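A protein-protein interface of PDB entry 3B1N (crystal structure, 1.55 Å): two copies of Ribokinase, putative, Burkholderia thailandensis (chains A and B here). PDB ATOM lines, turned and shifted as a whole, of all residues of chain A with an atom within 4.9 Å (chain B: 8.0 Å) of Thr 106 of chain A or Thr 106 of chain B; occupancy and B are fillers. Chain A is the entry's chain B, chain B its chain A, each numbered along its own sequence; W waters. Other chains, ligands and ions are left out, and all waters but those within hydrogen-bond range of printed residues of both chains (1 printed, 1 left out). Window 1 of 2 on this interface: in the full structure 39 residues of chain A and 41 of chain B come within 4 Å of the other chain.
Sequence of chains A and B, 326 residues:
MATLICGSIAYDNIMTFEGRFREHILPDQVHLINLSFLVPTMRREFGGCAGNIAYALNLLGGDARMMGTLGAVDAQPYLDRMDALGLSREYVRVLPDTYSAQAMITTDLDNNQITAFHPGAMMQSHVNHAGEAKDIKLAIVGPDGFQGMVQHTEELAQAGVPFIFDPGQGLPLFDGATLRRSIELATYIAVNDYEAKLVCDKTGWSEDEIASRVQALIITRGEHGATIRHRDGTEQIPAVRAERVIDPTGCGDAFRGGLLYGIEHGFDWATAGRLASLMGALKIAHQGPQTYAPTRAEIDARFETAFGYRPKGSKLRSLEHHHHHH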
ATOM      1  N   MET A  15      19.159  20.118  27.373  1.00  0.00           N
ATOM      2  CA  MET A  15      19.145  21.114  26.315  1.00  0.00           C
ATOM      3  C   MET A  15      18.948  20.363  25.021  1.00  0.00           C
ATOM      4  O   MET A  15      19.847  19.635  24.569  1.00  0.00           O
ATOM      5  CB  MET A  15      20.481  21.831  26.358  1.00  0.00           C
ATOM      6  CG  MET A  15      20.585  22.770  27.609  1.00  0.00           C
ATOM      7  SD  MET A  15      22.282  23.037  28.119  1.00  0.00           S
ATOM      8  CE  MET A  15      22.602  21.509  29.057  1.00  0.00           C
ATOM      9  N   PHE A  21      22.475  16.107  14.972  1.00  0.00           N
ATOM     10  CA  PHE A  21      23.919  16.457  14.836  1.00  0.00           C
ATOM     11  C   PHE A  21      24.547  15.996  13.532  1.00  0.00           C
ATOM     12  O   PHE A  21      25.391  16.662  12.986  1.00  0.00           O
ATOM     13  CB  PHE A  21      24.766  15.893  15.991  1.00  0.00           C
ATOM     14  CG  PHE A  21      24.356  16.368  17.362  1.00  0.00           C
ATOM     15  CD1 PHE A  21      23.857  17.625  17.579  1.00  0.00           C
ATOM     16  CD2 PHE A  21      24.585  15.514  18.475  1.00  0.00           C
ATOM     17  CE1 PHE A  21      23.455  18.094  18.886  1.00  0.00           C
ATOM     18  CE2 PHE A  21      24.222  15.962  19.784  1.00  0.00           C
ATOM     19  CZ  PHE A  21      23.651  17.213  19.988  1.00  0.00           C
ATOM     20  N   PHE A  37      21.775  27.461  19.921  1.00  0.00           N
ATOM     21  CA  PHE A  37      20.316  27.362  19.756  1.00  0.00           C
ATOM     22  C   PHE A  37      19.644  27.902  21.008  1.00  0.00           C
ATOM     23  O   PHE A  37      20.189  27.793  22.137  1.00  0.00           O
ATOM     24  CB  PHE A  37      19.884  25.926  19.422  1.00  0.00           C
ATOM     25  CG  PHE A  37      20.320  24.869  20.418  1.00  0.00           C
ATOM     26  CD1 PHE A  37      19.469  24.487  21.466  1.00  0.00           C
ATOM     27  CD2 PHE A  37      21.567  24.238  20.297  1.00  0.00           C
ATOM     28  CE1 PHE A  37      19.864  23.462  22.399  1.00  0.00           C
ATOM     29  CE2 PHE A  37      21.960  23.266  21.222  1.00  0.00           C
ATOM     30  CZ  PHE A  37      21.103  22.881  22.277  1.00  0.00           C
ATOM     31  N   MET A 104      24.434  18.031  32.801  1.00  0.00           N
ATOM     32  CA  MET A 104      24.072  19.023  31.795  1.00  0.00           C
ATOM     33  C   MET A 104      24.110  18.264  30.473  1.00  0.00           C
ATOM     34  O   MET A 104      25.164  17.844  30.029  1.00  0.00           O
ATOM     35  CB  MET A 104      25.080  20.200  31.821  1.00  0.00           C
ATOM     36  CG  MET A 104      25.232  20.897  33.172  1.00  0.00           C
ATOM     37  SD  MET A 104      23.844  22.018  33.472  1.00  0.00           S
ATOM     38  CE  MET A 104      23.964  23.159  32.104  1.00  0.00           C
ATOM     39  N   ILE A 105      22.934  17.988  29.927  1.00  0.00           N
ATOM     40  CA  ILE A 105      22.784  17.074  28.794  1.00  0.00           C
ATOM     41  C   ILE A 105      22.354  17.815  27.526  1.00  0.00           C
ATOM     42  O   ILE A 105      21.318  18.447  27.520  1.00  0.00           O
ATOM     43  CB  ILE A 105      21.669  16.039  29.165  1.00  0.00           C
ATOM     44  CG1 ILE A 105      22.008  15.357  30.487  1.00  0.00           C
ATOM     45  CG2 ILE A 105      21.418  15.012  27.993  1.00  0.00           C
ATOM     46  CD1 ILE A 105      20.847  14.395  31.000  1.00  0.00           C
ATOM     47  N   THR A 106      23.174  17.706  26.471  1.00  0.00           N
ATOM     48  CA  THR A 106      22.728  18.223  25.171  1.00  0.00           C
ATOM     49  C   THR A 106      22.316  17.111  24.244  1.00  0.00           C
ATOM     50  O   THR A 106      23.110  16.197  24.002  1.00  0.00           O
ATOM     51  CB  THR A 106      23.726  19.121  24.542  1.00  0.00           C
ATOM     52  OG1 THR A 106      24.045  20.155  25.465  1.00  0.00           O
ATOM     53  CG2 THR A 106      23.091  19.648  23.218  1.00  0.00           C
ATOM     54  N   THR A 107      21.039  17.102  23.852  1.00  0.00           N
ATOM     55  CA  THR A 107      20.529  16.017  23.050  1.00  0.00           C
ATOM     56  C   THR A 107      20.228  16.462  21.605  1.00  0.00           C
ATOM     57  O   THR A 107      20.057  17.653  21.365  1.00  0.00           O
ATOM     58  CB  THR A 107      19.285  15.342  23.762  1.00  0.00           C
ATOM     59  OG1 THR A 107      18.674  14.410  22.874  1.00  0.00           O
ATOM     60  CG2 THR A 107      18.245  16.366  24.247  1.00  0.00           C
ATOM     61  N   ASP A 108      20.194  15.515  20.697  1.00  0.00           N
ATOM     62  CA  ASP A 108      19.532  15.757  19.420  1.00  0.00           C
ATOM     63  C   ASP A 108      18.372  14.802  19.314  1.00  0.00           C
ATOM     64  O   ASP A 108      18.075  14.093  20.306  1.00  0.00           O
ATOM     65  CB  ASP A 108      20.471  15.711  18.201  1.00  0.00           C
ATOM     66  CG  ASP A 108      20.898  14.306  17.799  1.00  0.00           C
ATOM     67  OD1 ASP A 108      20.467  13.292  18.418  1.00  0.00           O
ATOM     68  OD2 ASP A 108      21.659  14.181  16.836  1.00  0.00           O
ATOM     69  N   ASN A 112      21.224  11.132  20.169  1.00  0.00           N
ATOM     70  CA  ASN A 112      22.617  11.421  20.548  1.00  0.00           C
ATOM     71  C   ASN A 112      22.600  12.322  21.749  1.00  0.00           C
ATOM     72  O   ASN A 112      21.722  13.192  21.838  1.00  0.00           O
ATOM     73  CB  ASN A 112      23.388  12.061  19.375  1.00  0.00           C
ATOM     74  CG  ASN A 112      23.460  11.128  18.197  1.00  0.00           C
ATOM     75  OD1 ASN A 112      23.882   9.984  18.345  1.00  0.00           O
ATOM     76  ND2 ASN A 112      22.992  11.581  17.009  1.00  0.00           N
ATOM     77  N   GLN A 113      23.509  12.068  22.702  1.00  0.00           N
ATOM     78  CA  GLN A 113      23.672  12.829  23.959  1.00  0.00           C
ATOM     79  C   GLN A 113      25.149  13.221  24.128  1.00  0.00           C
ATOM     80  O   GLN A 113      25.999  12.330  24.000  1.00  0.00           O
ATOM     81  CB  GLN A 113      23.288  11.945  25.174  1.00  0.00           C
ATOM     82  CG  GLN A 113      21.802  11.666  25.326  1.00  0.00           C
ATOM     83  CD  GLN A 113      21.408  10.888  26.603  1.00  0.00           C
ATOM     84  OE1 GLN A 113      21.725  11.272  27.738  1.00  0.00           O
ATOM     85  NE2 GLN A 113      20.658   9.809  26.406  1.00  0.00           N
ATOM     86  N   ILE A 114      25.468  14.487  24.443  1.00  0.00           N
ATOM     87  CA  ILE A 114      26.791  14.816  24.999  1.00  0.00           C
ATOM     88  C   ILE A 114      26.518  15.472  26.378  1.00  0.00           C
ATOM     89  O   ILE A 114      25.770  16.497  26.459  1.00  0.00           O
ATOM     90  CB  ILE A 114      27.589  15.790  24.108  1.00  0.00           C
ATOM     91  CG1 ILE A 114      27.830  15.141  22.746  1.00  0.00           C
ATOM     92  CG2 ILE A 114      28.941  16.172  24.834  1.00  0.00           C
ATOM     93  CD1 ILE A 114      28.524  16.107  21.710  1.00  0.00           C
ATOM     94  N   THR A 115      27.028  14.839  27.430  1.00  0.00           N
ATOM     95  CA  THR A 115      26.667  15.218  28.806  1.00  0.00           C
ATOM     96  C   THR A 115      27.915  15.626  29.592  1.00  0.00           C
ATOM     97  O   THR A 115      28.904  14.893  29.609  1.00  0.00           O
ATOM     98  CB  THR A 115      25.998  14.030  29.492  1.00  0.00           C
ATOM     99  OG1 THR A 115      24.756  13.766  28.829  1.00  0.00           O
ATOM    100  CG2 THR A 115      25.754  14.299  30.995  1.00  0.00           C
ATOM    101  N   ASN B  13      28.435  29.381  31.208  1.00  0.00           N
ATOM    102  CA  ASN B  13      28.673  28.165  31.930  1.00  0.00           C
ATOM    103  C   ASN B  13      29.280  27.234  30.924  1.00  0.00           C
ATOM    104  O   ASN B  13      28.557  26.762  30.019  1.00  0.00           O
ATOM    105  CB  ASN B  13      27.306  27.665  32.457  1.00  0.00           C
ATOM    106  CG  ASN B  13      26.516  28.803  33.153  1.00  0.00           C
ATOM    107  OD1 ASN B  13      26.802  29.122  34.318  1.00  0.00           O
ATOM    108  ND2 ASN B  13      25.618  29.514  32.394  1.00  0.00           N
ATOM    109  N   ILE B  14      30.581  26.982  31.029  1.00  0.00           N
ATOM    110  CA  ILE B  14      31.324  26.311  29.989  1.00  0.00           C
ATOM    111  C   ILE B  14      31.756  24.969  30.497  1.00  0.00           C
ATOM    112  O   ILE B  14      32.372  24.870  31.615  1.00  0.00           O
ATOM    113  CB  ILE B  14      32.585  27.128  29.620  1.00  0.00           C
ATOM    114  CG1 ILE B  14      32.157  28.462  29.049  1.00  0.00           C
ATOM    115  CG2 ILE B  14      33.448  26.323  28.615  1.00  0.00           C
ATOM    116  CD1 ILE B  14      33.261  29.500  29.023  1.00  0.00           C
ATOM    117  N   MET B  15      31.444  23.937  29.721  1.00  0.00           N
ATOM    118  CA  MET B  15      31.794  22.589  30.050  1.00  0.00           C
ATOM    119  C   MET B  15      32.736  22.099  28.955  1.00  0.00           C
ATOM    120  O   MET B  15      32.312  21.712  27.837  1.00  0.00           O
ATOM    121  CB  MET B  15      30.509  21.769  30.168  1.00  0.00           C
ATOM    122  CG  MET B  15      29.603  22.250  31.336  1.00  0.00           C
ATOM    123  SD  MET B  15      27.835  22.073  31.026  1.00  0.00           S
ATOM    124  CE  MET B  15      27.537  23.396  29.833  1.00  0.00           C
ATOM    125  N   THR B  16      34.032  22.109  29.240  1.00  0.00           N
ATOM    126  CA  THR B  16      35.013  21.760  28.224  1.00  0.00           C
ATOM    127  C   THR B  16      35.455  20.325  28.382  1.00  0.00           C
ATOM    128  O   THR B  16      36.116  19.981  29.411  1.00  0.00           O
ATOM    129  CB  THR B  16      36.261  22.702  28.356  1.00  0.00           C
ATOM    130  OG1 THR B  16      35.831  24.055  28.342  1.00  0.00           O
ATOM    131  CG2 THR B  16      37.345  22.390  27.264  1.00  0.00           C
ATOM    132  N   PHE B  17      35.171  19.505  27.378  1.00  0.00           N
ATOM    133  CA  PHE B  17      35.631  18.132  27.345  1.00  0.00           C
ATOM    134  C   PHE B  17      37.144  18.140  27.124  1.00  0.00           C
ATOM    135  O   PHE B  17      37.655  18.724  26.149  1.00  0.00           O
ATOM    136  CB  PHE B  17      34.888  17.362  26.242  1.00  0.00           C
ATOM    137  CG  PHE B  17      35.388  15.977  26.019  1.00  0.00           C
ATOM    138  CD1 PHE B  17      35.548  15.106  27.090  1.00  0.00           C
ATOM    139  CD2 PHE B  17      35.641  15.530  24.732  1.00  0.00           C
ATOM    140  CE1 PHE B  17      35.963  13.772  26.874  1.00  0.00           C
ATOM    141  CE2 PHE B  17      36.074  14.205  24.498  1.00  0.00           C
ATOM    142  CZ  PHE B  17      36.243  13.334  25.608  1.00  0.00           C
ATOM    143  N   PHE B  21      35.700  15.668  20.403  1.00  0.00           N
ATOM    144  CA  PHE B  21      34.480  14.929  20.016  1.00  0.00           C
ATOM    145  C   PHE B  21      34.712  14.121  18.727  1.00  0.00           C
ATOM    146  O   PHE B  21      34.123  13.059  18.542  1.00  0.00           O
ATOM    147  CB  PHE B  21      33.335  15.900  19.751  1.00  0.00           C
ATOM    148  CG  PHE B  21      32.899  16.729  20.939  1.00  0.00           C
ATOM    149  CD1 PHE B  21      32.958  16.266  22.258  1.00  0.00           C
ATOM    150  CD2 PHE B  21      32.308  18.002  20.725  1.00  0.00           C
ATOM    151  CE1 PHE B  21      32.507  17.040  23.302  1.00  0.00           C
ATOM    152  CE2 PHE B  21      31.866  18.769  21.776  1.00  0.00           C
ATOM    153  CZ  PHE B  21      31.977  18.300  23.086  1.00  0.00           C
ATOM    154  N   ILE B  33      26.899   9.534  18.650  1.00  0.00           N
ATOM    155  CA  ILE B  33      27.746   9.914  19.770  1.00  0.00           C
ATOM    156  C   ILE B  33      26.968   9.875  21.067  1.00  0.00           C
ATOM    157  O   ILE B  33      25.822  10.339  21.163  1.00  0.00           O
ATOM    158  CB  ILE B  33      28.474  11.272  19.542  1.00  0.00           C
ATOM    159  CG1 ILE B  33      29.432  11.538  20.716  1.00  0.00           C
ATOM    160  CG2 ILE B  33      27.478  12.405  19.406  1.00  0.00           C
ATOM    161  CD1 ILE B  33      30.443  12.655  20.523  1.00  0.00           C
ATOM    162  N   LEU B  35      28.455  10.622  24.957  1.00  0.00           N
ATOM    163  CA  LEU B  35      29.598  10.917  25.695  1.00  0.00           C
ATOM    164  C   LEU B  35      29.110  11.573  26.971  1.00  0.00           C
ATOM    165  O   LEU B  35      28.352  12.496  26.944  1.00  0.00           O
ATOM    166  CB  LEU B  35      30.470  11.857  24.859  1.00  0.00           C
ATOM    167  CG  LEU B  35      31.747  12.365  25.461  1.00  0.00           C
ATOM    168  CD1 LEU B  35      32.684  11.236  25.906  1.00  0.00           C
ATOM    169  CD2 LEU B  35      32.372  13.241  24.364  1.00  0.00           C
ATOM    170  N   PHE B  37      31.156  13.220  30.297  1.00  0.00           N
ATOM    171  CA  PHE B  37      32.480  13.525  30.837  1.00  0.00           C
ATOM    172  C   PHE B  37      32.335  14.269  32.139  1.00  0.00           C
ATOM    173  O   PHE B  37      31.405  15.058  32.294  1.00  0.00           O
ATOM    174  CB  PHE B  37      33.370  14.326  29.820  1.00  0.00           C
ATOM    175  CG  PHE B  37      32.787  15.633  29.345  1.00  0.00           C
ATOM    176  CD1 PHE B  37      33.191  16.881  29.928  1.00  0.00           C
ATOM    177  CD2 PHE B  37      31.895  15.679  28.299  1.00  0.00           C
ATOM    178  CE1 PHE B  37      32.659  18.105  29.472  1.00  0.00           C
ATOM    179  CE2 PHE B  37      31.379  16.891  27.826  1.00  0.00           C
ATOM    180  CZ  PHE B  37      31.764  18.117  28.407  1.00  0.00           C
ATOM    181  N   ALA B 103      24.829  31.682  28.563  1.00  0.00           N
ATOM    182  CA  ALA B 103      25.214  30.640  27.606  1.00  0.00           C
ATOM    183  C   ALA B 103      25.623  29.368  28.299  1.00  0.00           C
ATOM    184  O   ALA B 103      26.468  29.394  29.175  1.00  0.00           O
ATOM    185  CB  ALA B 103      26.401  31.109  26.753  1.00  0.00           C
ATOM    186  N   MET B 104      25.070  28.226  27.896  1.00  0.00           N
ATOM    187  CA  MET B 104      25.549  26.944  28.394  1.00  0.00           C
ATOM    188  C   MET B 104      26.274  26.298  27.283  1.00  0.00           C
ATOM    189  O   MET B 104      25.667  25.869  26.282  1.00  0.00           O
ATOM    190  CB  MET B 104      24.399  26.026  28.830  1.00  0.00           C
ATOM    191  CG  MET B 104      23.222  26.699  29.314  1.00  0.00           C
ATOM    192  SD  MET B 104      23.419  27.890  30.621  1.00  0.00           S
ATOM    193  CE  MET B 104      24.116  26.671  31.716  1.00  0.00           C
ATOM    194  N   ILE B 105      27.597  26.210  27.413  1.00  0.00           N
ATOM    195  CA  ILE B 105      28.428  25.865  26.275  1.00  0.00           C
ATOM    196  C   ILE B 105      29.110  24.533  26.529  1.00  0.00           C
ATOM    197  O   ILE B 105      29.861  24.408  27.511  1.00  0.00           O
ATOM    198  CB  ILE B 105      29.542  26.929  26.110  1.00  0.00           C
ATOM    199  CG1 ILE B 105      28.910  28.296  25.836  1.00  0.00           C
ATOM    200  CG2 ILE B 105      30.475  26.536  24.982  1.00  0.00           C
ATOM    201  CD1 ILE B 105      29.920  29.439  25.748  1.00  0.00           C
ATOM    202  N   THR B 106      28.814  23.537  25.716  1.00  0.00           N
ATOM    203  CA  THR B 106      29.403  22.219  25.761  1.00  0.00           C
ATOM    204  C   THR B 106      30.379  22.154  24.618  1.00  0.00           C
ATOM    205  O   THR B 106      30.013  22.344  23.457  1.00  0.00           O
ATOM    206  CB  THR B 106      28.316  21.121  25.669  1.00  0.00           C
ATOM    207  OG1 THR B 106      27.499  21.244  26.859  1.00  0.00           O
ATOM    208  CG2 THR B 106      28.965  19.767  25.618  1.00  0.00           C
ATOM    209  N   THR B 107      31.633  21.907  24.905  1.00  0.00           N
ATOM    210  CA  THR B 107      32.661  22.054  23.899  1.00  0.00           C
ATOM    211  C   THR B 107      33.829  21.120  24.137  1.00  0.00           C
ATOM    212  O   THR B 107      33.790  20.299  25.113  1.00  0.00           O
ATOM    213  CB  THR B 107      33.120  23.520  23.896  1.00  0.00           C
ATOM    214  OG1 THR B 107      33.934  23.769  22.753  1.00  0.00           O
ATOM    215  CG2 THR B 107      33.924  23.860  25.173  1.00  0.00           C
ATOM    216  N   ASP B 108      34.840  21.212  23.272  1.00  0.00           N
ATOM    217  CA  ASP B 108      35.982  20.285  23.326  1.00  0.00           C
ATOM    218  C   ASP B 108      37.263  21.084  23.019  1.00  0.00           C
ATOM    219  O   ASP B 108      37.180  22.305  22.878  1.00  0.00           O
ATOM    220  CB  ASP B 108      35.812  19.023  22.433  1.00  0.00           C
ATOM    221  CG  ASP B 108      35.905  19.321  20.946  1.00  0.00           C
ATOM    222  OD1 ASP B 108      36.111  20.527  20.596  1.00  0.00           O
ATOM    223  OD2 ASP B 108      35.822  18.377  20.149  1.00  0.00           O
ATOM    224  N   ASN B 111      37.331  23.335  19.980  1.00  0.00           N
ATOM    225  CA  ASN B 111      36.412  24.492  19.919  1.00  0.00           C
ATOM    226  C   ASN B 111      35.136  24.180  19.149  1.00  0.00           C
ATOM    227  O   ASN B 111      34.550  25.063  18.524  1.00  0.00           O
ATOM    228  CB  ASN B 111      37.090  25.744  19.323  1.00  0.00           C
ATOM    229  CG  ASN B 111      36.589  27.043  19.924  1.00  0.00           C
ATOM    230  OD1 ASN B 111      35.734  27.051  20.823  1.00  0.00           O
ATOM    231  ND2 ASN B 111      37.139  28.162  19.433  1.00  0.00           N
ATOM    232  N   ASN B 112      34.686  22.935  19.274  1.00  0.00           N
ATOM    233  CA  ASN B 112      33.360  22.502  18.760  1.00  0.00           C
ATOM    234  C   ASN B 112      32.245  22.894  19.698  1.00  0.00           C
ATOM    235  O   ASN B 112      31.645  22.004  20.353  1.00  0.00           O
ATOM    236  CB  ASN B 112      33.393  20.988  18.534  1.00  0.00           C
ATOM    237  CG  ASN B 112      34.284  20.618  17.367  1.00  0.00           C
ATOM    238  OD1 ASN B 112      34.249  21.277  16.315  1.00  0.00           O
ATOM    239  ND2 ASN B 112      35.063  19.547  17.505  1.00  0.00           N
ATOM    240  N   GLN B 113      31.912  24.188  19.773  1.00  0.00           N
ATOM    241  CA  GLN B 113      30.976  24.714  20.723  1.00  0.00           C
ATOM    242  C   GLN B 113      29.562  24.372  20.332  1.00  0.00           C
ATOM    243  O   GLN B 113      29.099  24.807  19.263  1.00  0.00           O
ATOM    244  CB  GLN B 113      31.034  26.262  20.913  1.00  0.00           C
ATOM    245  CG  GLN B 113      32.343  26.718  21.522  1.00  0.00           C
ATOM    246  CD  GLN B 113      32.420  28.214  21.687  1.00  0.00           C
ATOM    247  OE1 GLN B 113      31.436  28.865  22.040  1.00  0.00           O
ATOM    248  NE2 GLN B 113      33.595  28.773  21.437  1.00  0.00           N
ATOM    249  N   ILE B 114      28.889  23.648  21.225  1.00  0.00           N
ATOM    250  CA  ILE B 114      27.440  23.375  21.097  1.00  0.00           C
ATOM    251  C   ILE B 114      26.777  24.066  22.220  1.00  0.00           C
ATOM    252  O   ILE B 114      26.873  23.639  23.402  1.00  0.00           O
ATOM    253  CB  ILE B 114      27.196  21.874  21.119  1.00  0.00           C
ATOM    254  CG1 ILE B 114      27.928  21.207  19.963  1.00  0.00           C
ATOM    255  CG2 ILE B 114      25.656  21.559  21.131  1.00  0.00           C
ATOM    256  CD1 ILE B 114      27.882  19.628  20.022  1.00  0.00           C
ATOM    257  N   THR B 115      26.126  25.167  21.904  1.00  0.00           N
ATOM    258  CA  THR B 115      25.653  26.093  22.944  1.00  0.00           C
ATOM    259  C   THR B 115      24.141  26.206  23.022  1.00  0.00           C
ATOM    260  O   THR B 115      23.450  26.411  22.002  1.00  0.00           O
ATOM    261  CB  THR B 115      26.219  27.492  22.712  1.00  0.00           C
ATOM    262  OG1 THR B 115      27.662  27.387  22.801  1.00  0.00           O
ATOM    263  CG2 THR B 115      25.716  28.499  23.741  1.00  0.00           C
ATOM    264  N   ALA B 116      23.639  26.079  24.240  1.00  0.00           N
ATOM    265  CA  ALA B 116      22.262  26.370  24.546  1.00  0.00           C
ATOM    266  C   ALA B 116      22.227  27.789  25.120  1.00  0.00           C
ATOM    267  O   ALA B 116      22.813  28.054  26.185  1.00  0.00           O
ATOM    268  CB  ALA B 116      21.760  25.361  25.537  1.00  0.00           C
ATOM    269  N   THR B 249      37.202  28.309  24.328  1.00  0.00           N
ATOM    270  CA  THR B 249      36.003  29.140  24.276  1.00  0.00           C
ATOM    271  C   THR B 249      36.382  30.621  24.412  1.00  0.00           C
ATOM    272  O   THR B 249      37.016  31.012  25.393  1.00  0.00           O
ATOM    273  CB  THR B 249      35.065  28.791  25.471  1.00  0.00           C
ATOM    274  OG1 THR B 249      34.856  27.385  25.467  1.00  0.00           O
ATOM    275  CG2 THR B 249      33.704  29.534  25.305  1.00  0.00           C
HETATM  276  O   HOH W   1      25.715  19.339  27.384  1.00  0.00           O
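N of Leu 35 of chain B sits at hydrogen-bond distance from O of Gln 113 of chain A, 3.1 Å away.
N of Phe 37 of chain B sits at hydrogen-bond distance from O of Thr 115 of chain A, at 2.9 Å.
The backbone carbonyl oxygen of Leu 35 of chain B is in hydrogen-bond range of the backbone NH of Thr 115 of chain A, at 2.7 Å.
The side-chain amide oxygen of Asn 112 of chain A is in hydrogen-bond range of the backbone NH of Ile 33 of chain B.
N of Phe 37 of chain A lies within hydrogen-bond range of O of Thr 115 of chain B, at 2.9 Å.
N of Gln 113 of chain A lies within hydrogen-bond range of O of Ile 33 of chain B (3.3 Å).
The backbone carbonyl oxygen of Asn 112 of chain A sits close to the side-chain hydroxyl of Thr 107 of chain A (3.4 Å).
O of Met 15 of chain A lies within hydrogen-bond range of N of Thr 107 of chain A.
The backbone NH of Thr 106 of chain A is in hydrogen-bond range of the backbone carbonyl oxygen of Ile 114 of chain A (2.9 Å).
The backbone NH (N) of Met 104 of chain B is in hydrogen-bond range of the backbone carbonyl oxygen (O) of Ala 116 of chain B (2.8 Å).
O of Ile 105 of chain B is in hydrogen-bond range of N of Met 15 of chain B (2.8 Å).
O of Ile 105 of chain A is in hydrogen-bond range of N of Met 15 of chain A.
Met 15 of chain A touches Met 104 of chain B.
Ala 116 of chain B touches Phe 37 of chain A.
Met 15 of chain B touches Met 104 of chain A (SD to CB, 3.4 Å).
Thr 106 of chain A touches Thr 106 of chain B (OG1 to OG1, 3.9 Å).
CG2 of Ile 114 of chain B touches CG2 of Thr 106 of chain A, at 3.8 Å.
Ile 114 of chain A touches Phe 21 of chain B.
O of Leu 35 of chain B touches CA of Ile 114 of chain A, at 3.4 Å.
CE2 of Phe 37 of chain B touches CG2 of Ile 114 of chain A (3.9 Å).
Ile 114 of chain A touches Thr 106 of chain B.
Ile 114 of chain B touches Ile 114 of chain A.
Thr 106 of chain A touches two residues of chain B.
Thr 106 of chain B touches two residues of chain A.
Of the printed residues of chain A, Phe 21 of chain B touches Ile 114 (3.98 Å).
Printed residues of chain A within 4 Å of Ile 33 of chain B: Asn 112 and Gln 113.
Printed residues of chain A within 4 Å of Met 15 of chain B: Met 104 (3.4 Å).
Printed residues of chain B within 4 Å of Phe 37 of chain A: Thr 115 and Ala 116.
Printed residues of chain B within 4 Å of Ile 114 of chain A: Phe 21, Leu 35, Phe 37, Thr 106 and Ile 114.
Asn 112 of chain B touches none of the printed residues of chain A.
Asn 111 of chain B touches none of the printed residues of chain A.
The nearest printed residue of chain A that does not touch Thr 106 of chain B is Met 104 of chain A (5.2 Å).
Printed residues of chain A that touch a printed residue of chain B: Met 15, Phe 37, Met 104, Thr 106, Asn 112, Gln 113, Ile 114 and Thr 115.
Hydrophobic or aromatic side chains of chain A within 4 Å of the printed part of chain B: Met 15, Phe 37, Met 104 and Ile 114.
Of the 22 printed residues of chain B, 10 touch a printed residue of chain A.
Hydrophobic or aromatic side chains of chain B within 4 Å of the printed part of chain A: Met 15, Phe 21, Phe 37, Met 104, Ile 114 and Ala 116.
Among the printed residues, no Asp or Glu carboxylate lies within 4 Å of a Lys or Arg side-chain nitrogen of the other chain.
Met 15 of chain A touches Met 104 of chain B, and with the chains exchanged Met 104 of chain A touches Met 15 of chain B.
Met 104 of chain B touches its own counterpart, Met 104 of chain A.
Ile 114 of chain A touches Phe 21 of chain B, but with the chains exchanged Phe 21 of chain A does not touch Ile 114 of chain B (4.7 Å).
Ile 114 of chain A touches Phe 37 of chain B, but with the chains exchanged Phe 37 of chain A does not touch Ile 114 of chain B (4.1 Å).
Of the 18 pairs that touch across the chains among the printed residues, 9 have their exchanged pair printed and touching as well.
Water W1 lies within hydrogen-bond range of OG1 of Thr 106 of chain B, OG1 of Thr 106 of chain A, O of Ile 114 of chain A and O of Met 104 of chain A.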
